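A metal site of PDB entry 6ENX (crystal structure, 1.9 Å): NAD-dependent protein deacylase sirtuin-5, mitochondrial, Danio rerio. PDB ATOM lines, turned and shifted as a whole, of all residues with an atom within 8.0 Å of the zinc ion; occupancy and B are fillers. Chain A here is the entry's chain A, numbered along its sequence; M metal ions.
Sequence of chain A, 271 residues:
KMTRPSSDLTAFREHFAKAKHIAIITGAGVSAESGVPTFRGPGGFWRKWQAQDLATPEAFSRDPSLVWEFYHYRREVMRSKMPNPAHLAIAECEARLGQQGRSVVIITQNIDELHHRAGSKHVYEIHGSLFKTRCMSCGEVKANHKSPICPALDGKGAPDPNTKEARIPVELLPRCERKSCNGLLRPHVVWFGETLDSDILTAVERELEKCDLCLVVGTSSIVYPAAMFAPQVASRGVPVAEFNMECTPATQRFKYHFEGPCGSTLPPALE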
ATOM      1  N   ARG A 134      21.943  24.093   9.545  1.00  0.00           N
ATOM      2  CA  ARG A 134      22.236  23.269  10.708  1.00  0.00           C
ATOM      3  C   ARG A 134      20.980  22.463  11.081  1.00  0.00           C
ATOM      4  O   ARG A 134      19.907  23.023  11.087  1.00  0.00           O
ATOM      5  CB  ARG A 134      22.745  24.074  11.893  1.00  0.00           C
ATOM      6  CG  ARG A 134      23.043  23.144  13.062  1.00  0.00           C
ATOM      7  CD  ARG A 134      23.930  23.697  14.116  1.00  0.00           C
ATOM      8  NE  ARG A 134      23.284  24.635  15.045  1.00  0.00           N
ATOM      9  CZ  ARG A 134      23.318  25.983  14.993  1.00  0.00           C
ATOM     10  NH1 ARG A 134      23.884  26.633  13.979  1.00  0.00           N
ATOM     11  NH2 ARG A 134      22.758  26.700  15.967  1.00  0.00           N
ATOM     12  N   CYS A 135      21.137  21.163  11.318  1.00  0.00           N
ATOM     13  CA  CYS A 135      20.009  20.298  11.688  1.00  0.00           C
ATOM     14  C   CYS A 135      19.705  20.417  13.166  1.00  0.00           C
ATOM     15  O   CYS A 135      20.605  20.361  13.978  1.00  0.00           O
ATOM     16  CB  CYS A 135      20.297  18.828  11.331  1.00  0.00           C
ATOM     17  SG  CYS A 135      18.988  17.672  11.787  1.00  0.00           S
ATOM     18  N   MET A 136      18.419  20.570  13.504  1.00  0.00           N
ATOM     19  CA  MET A 136      17.976  20.747  14.874  1.00  0.00           C
ATOM     20  C   MET A 136      18.027  19.455  15.704  1.00  0.00           C
ATOM     21  O   MET A 136      17.955  19.551  16.925  1.00  0.00           O
ATOM     22  CB  MET A 136      16.574  21.318  14.940  1.00  0.00           C
ATOM     23  CG  MET A 136      16.464  22.735  14.408  1.00  0.00           C
ATOM     24  SD  MET A 136      17.352  23.968  15.340  1.00  0.00           S
ATOM     25  CE  MET A 136      16.162  24.406  16.628  1.00  0.00           C
ATOM     26  N   SER A 137      18.151  18.304  15.051  1.00  0.00           N
ATOM     27  CA  SER A 137      18.105  16.998  15.704  1.00  0.00           C
ATOM     28  C   SER A 137      19.488  16.445  15.781  1.00  0.00           C
ATOM     29  O   SER A 137      19.975  16.207  16.847  1.00  0.00           O
ATOM     30  CB  SER A 137      17.253  16.021  14.898  1.00  0.00           C
ATOM     31  OG  SER A 137      15.909  16.456  14.847  1.00  0.00           O
ATOM     32  N   CYS A 138      20.123  16.248  14.627  1.00  0.00           N
ATOM     33  CA  CYS A 138      21.427  15.616  14.589  1.00  0.00           C
ATOM     34  C   CYS A 138      22.599  16.619  14.633  1.00  0.00           C
ATOM     35  O   CYS A 138      23.714  16.218  14.862  1.00  0.00           O
ATOM     36  CB  CYS A 138      21.508  14.687  13.379  1.00  0.00           C
ATOM     37  SG  CYS A 138      21.858  15.475  11.800  1.00  0.00           S
ATOM     38  N   GLY A 139      22.364  17.902  14.391  1.00  0.00           N
ATOM     39  CA  GLY A 139      23.457  18.884  14.460  1.00  0.00           C
ATOM     40  C   GLY A 139      24.353  19.017  13.228  1.00  0.00           C
ATOM     41  O   GLY A 139      25.240  19.881  13.202  1.00  0.00           O
ATOM     42  N   GLU A 140      24.104  18.224  12.195  1.00  0.00           N
ATOM     43  CA  GLU A 140      24.857  18.252  10.954  1.00  0.00           C
ATOM     44  C   GLU A 140      24.866  19.675  10.376  1.00  0.00           C
ATOM     45  O   GLU A 140      23.807  20.303  10.300  1.00  0.00           O
ATOM     46  CB  GLU A 140      24.170  17.270   9.981  1.00  0.00           C
ATOM     47  CG  GLU A 140      24.373  17.436   8.496  1.00  0.00           C
ATOM     48  CD  GLU A 140      25.679  16.850   7.991  1.00  0.00           C
ATOM     49  OE1 GLU A 140      26.652  16.836   8.761  1.00  0.00           O
ATOM     50  OE2 GLU A 140      25.696  16.419   6.804  1.00  0.00           O
ATOM     51  N   VAL A 141      26.048  20.201  10.044  1.00  0.00           N
ATOM     52  CA  VAL A 141      26.226  21.461   9.289  1.00  0.00           C
ATOM     53  C   VAL A 141      26.644  21.167   7.831  1.00  0.00           C
ATOM     54  O   VAL A 141      27.508  20.322   7.599  1.00  0.00           O
ATOM     55  CB  VAL A 141      27.242  22.395   9.974  1.00  0.00           C
ATOM     56  CG1 VAL A 141      27.478  23.682   9.164  1.00  0.00           C
ATOM     57  CG2 VAL A 141      26.709  22.731  11.352  1.00  0.00           C
ATOM     58  N   ARG A 175      14.267  20.206   5.696  1.00  0.00           N
ATOM     59  CA  ARG A 175      14.504  19.077   6.544  1.00  0.00           C
ATOM     60  C   ARG A 175      15.853  18.508   6.204  1.00  0.00           C
ATOM     61  O   ARG A 175      16.254  18.544   5.072  1.00  0.00           O
ATOM     62  CB  ARG A 175      13.459  17.975   6.280  1.00  0.00           C
ATOM     63  CG  ARG A 175      11.981  18.400   6.354  1.00  0.00           C
ATOM     64  CD  ARG A 175      11.589  19.110   7.635  1.00  0.00           C
ATOM     65  NE  ARG A 175      11.662  18.247   8.805  1.00  0.00           N
ATOM     66  CZ  ARG A 175      11.023  18.452   9.970  1.00  0.00           C
ATOM     67  NH1 ARG A 175      10.244  19.514  10.174  1.00  0.00           N
ATOM     68  NH2 ARG A 175      11.181  17.598  10.963  1.00  0.00           N
ATOM     69  N   CYS A 176      16.468  17.897   7.195  1.00  0.00           N
ATOM     70  CA  CYS A 176      17.730  17.165   7.062  1.00  0.00           C
ATOM     71  C   CYS A 176      17.644  15.963   6.092  1.00  0.00           C
ATOM     72  O   CYS A 176      16.837  15.077   6.278  1.00  0.00           O
ATOM     73  CB  CYS A 176      18.110  16.646   8.440  1.00  0.00           C
ATOM     74  SG  CYS A 176      19.709  15.834   8.571  1.00  0.00           S
ATOM     75  N   GLU A 177      18.488  15.956   5.061  1.00  0.00           N
ATOM     76  CA  GLU A 177      18.421  14.919   4.033  1.00  0.00           C
ATOM     77  C   GLU A 177      19.342  13.731   4.332  1.00  0.00           C
ATOM     78  O   GLU A 177      19.323  12.725   3.633  1.00  0.00           O
ATOM     79  CB  GLU A 177      18.679  15.530   2.670  1.00  0.00           C
ATOM     80  CG  GLU A 177      17.558  16.494   2.283  1.00  0.00           C
ATOM     81  CD  GLU A 177      17.553  16.851   0.806  1.00  0.00           C
ATOM     82  OE1 GLU A 177      18.638  17.051   0.225  1.00  0.00           O
ATOM     83  OE2 GLU A 177      16.434  16.928   0.231  1.00  0.00           O
ATOM     84  N   ARG A 178      20.108  13.840   5.414  1.00  0.00           N
ATOM     85  CA  ARG A 178      20.769  12.679   6.030  1.00  0.00           C
ATOM     86  C   ARG A 178      19.822  11.512   6.164  1.00  0.00           C
ATOM     87  O   ARG A 178      18.684  11.640   6.625  1.00  0.00           O
ATOM     88  CB  ARG A 178      21.257  13.045   7.429  1.00  0.00           C
ATOM     89  CG  ARG A 178      22.484  12.336   7.883  1.00  0.00           C
ATOM     90  CD  ARG A 178      23.447  13.346   8.486  1.00  0.00           C
ATOM     91  NE  ARG A 178      24.618  12.619   8.926  1.00  0.00           N
ATOM     92  CZ  ARG A 178      24.982  12.409  10.183  1.00  0.00           C
ATOM     93  NH1 ARG A 178      26.067  11.676  10.407  1.00  0.00           N
ATOM     94  NH2 ARG A 178      24.329  12.958  11.211  1.00  0.00           N
ATOM     95  N   LYS A 179      20.312  10.343   5.795  1.00  0.00           N
ATOM     96  CA  LYS A 179      19.504   9.147   5.789  1.00  0.00           C
ATOM     97  C   LYS A 179      19.246   8.812   7.259  1.00  0.00           C
ATOM     98  O   LYS A 179      20.210   8.642   8.048  1.00  0.00           O
ATOM     99  CB  LYS A 179      20.251   8.030   5.051  1.00  0.00           C
ATOM    100  CG  LYS A 179      20.762   8.416   3.657  1.00  0.00           C
ATOM    101  CD  LYS A 179      19.904   7.897   2.498  1.00  0.00           C
ATOM    102  CE  LYS A 179      20.757   7.703   1.271  1.00  0.00           C
ATOM    103  NZ  LYS A 179      20.043   6.970   0.189  1.00  0.00           N
ATOM    104  N   SER A 180      17.953   8.799   7.615  1.00  0.00           N
ATOM    105  CA  SER A 180      17.383   8.389   8.933  1.00  0.00           C
ATOM    106  C   SER A 180      17.236   9.523   9.936  1.00  0.00           C
ATOM    107  O   SER A 180      17.057   9.242  11.114  1.00  0.00           O
ATOM    108  CB  SER A 180      18.146   7.225   9.624  1.00  0.00           C
ATOM    109  OG  SER A 180      18.410   6.151   8.754  1.00  0.00           O
ATOM    110  N   CYS A 181      17.285  10.774   9.488  1.00  0.00           N
ATOM    111  CA  CYS A 181      17.091  11.912  10.400  1.00  0.00           C
ATOM    112  C   CYS A 181      15.767  12.681  10.212  1.00  0.00           C
ATOM    113  O   CYS A 181      14.925  12.766  11.132  1.00  0.00           O
ATOM    114  CB  CYS A 181      18.269  12.855  10.244  1.00  0.00           C
ATOM    115  SG  CYS A 181      18.162  14.200  11.398  1.00  0.00           S
ATOM    116  N   ASN A 182      15.601  13.295   9.056  1.00  0.00           N
ATOM    117  CA  ASN A 182      14.493  14.245   8.830  1.00  0.00           C
ATOM    118  C   ASN A 182      14.290  15.406   9.875  1.00  0.00           C
ATOM    119  O   ASN A 182      13.213  15.987   9.964  1.00  0.00           O
ATOM    120  CB  ASN A 182      13.185  13.440   8.676  1.00  0.00           C
ATOM    121  CG  ASN A 182      12.108  14.233   7.976  1.00  0.00           C
ATOM    122  OD1 ASN A 182      12.221  14.525   6.777  1.00  0.00           O
ATOM    123  ND2 ASN A 182      11.079  14.644   8.730  1.00  0.00           N
ATOM    124  N   GLY A 183      15.312  15.795  10.650  1.00  0.00           N
ATOM    125  CA  GLY A 183      15.138  16.858  11.632  1.00  0.00           C
ATOM    126  C   GLY A 183      14.890  18.172  10.899  1.00  0.00           C
ATOM    127  O   GLY A 183      15.177  18.303   9.706  1.00  0.00           O
ATOM    128  N   LEU A 184      14.343  19.152  11.605  1.00  0.00           N
ATOM    129  CA  LEU A 184      14.151  20.476  11.058  1.00  0.00           C
ATOM    130  C   LEU A 184      15.508  21.151  10.923  1.00  0.00           C
ATOM    131  O   LEU A 184      16.310  21.077  11.850  1.00  0.00           O
ATOM    132  CB  LEU A 184      13.229  21.327  11.965  1.00  0.00           C
ATOM    133  CG  LEU A 184      12.975  22.809  11.608  1.00  0.00           C
ATOM    134  CD1 LEU A 184      12.424  23.012  10.192  1.00  0.00           C
ATOM    135  CD2 LEU A 184      12.076  23.465  12.682  1.00  0.00           C
ATOM    136  N   LEU A 185      15.762  21.808   9.788  1.00  0.00           N
ATOM    137  CA  LEU A 185      16.977  22.613   9.656  1.00  0.00           C
ATOM    138  C   LEU A 185      16.680  24.047  10.017  1.00  0.00           C
ATOM    139  O   LEU A 185      15.524  24.502   9.925  1.00  0.00           O
ATOM    140  CB  LEU A 185      17.524  22.612   8.201  1.00  0.00           C
ATOM    141  CG  LEU A 185      17.749  21.218   7.641  1.00  0.00           C
ATOM    142  CD1 LEU A 185      18.139  21.416   6.197  1.00  0.00           C
ATOM    143  CD2 LEU A 185      18.786  20.455   8.425  1.00  0.00           C
HETATM  144 ZN    ZN M   1      19.789  15.712  10.829  1.00  0.00          ZN
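SG of Cys 181 lies close to N of Gly 183 (3.4 Å). The side-chain sulfur (SG) of Cys 176 lies close to the backbone NH (N) of Arg 178, 3.8 Å away. The backbone NH (N) of Cys 135 sits at hydrogen-bond distance from the backbone carbonyl oxygen (O) of Glu 140, 3.0 Å away. SG of Cys 138 sits close to N of Glu 140, 3.6 Å away. SG of Cys 135 sits close to N of Ser 137 (3.4 Å). N of Cys 176 is in hydrogen-bond range of O of Gly 183, 2.9 Å away. The side-chain sulfur (SG) of Cys 138 sits close to the guanidinium group (NH2) of Arg 178.
Within 4 Å of the zinc ion: Cys 135, Cys 138, Cys 176 and Cys 181. The nearest printed residue that does not touch the zinc ion is Gly 183 (4.5 Å).
The zinc ion is bound by SG of Cys 176, SG of Cys 181, SG of Cys 138 and SG of Cys 135.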
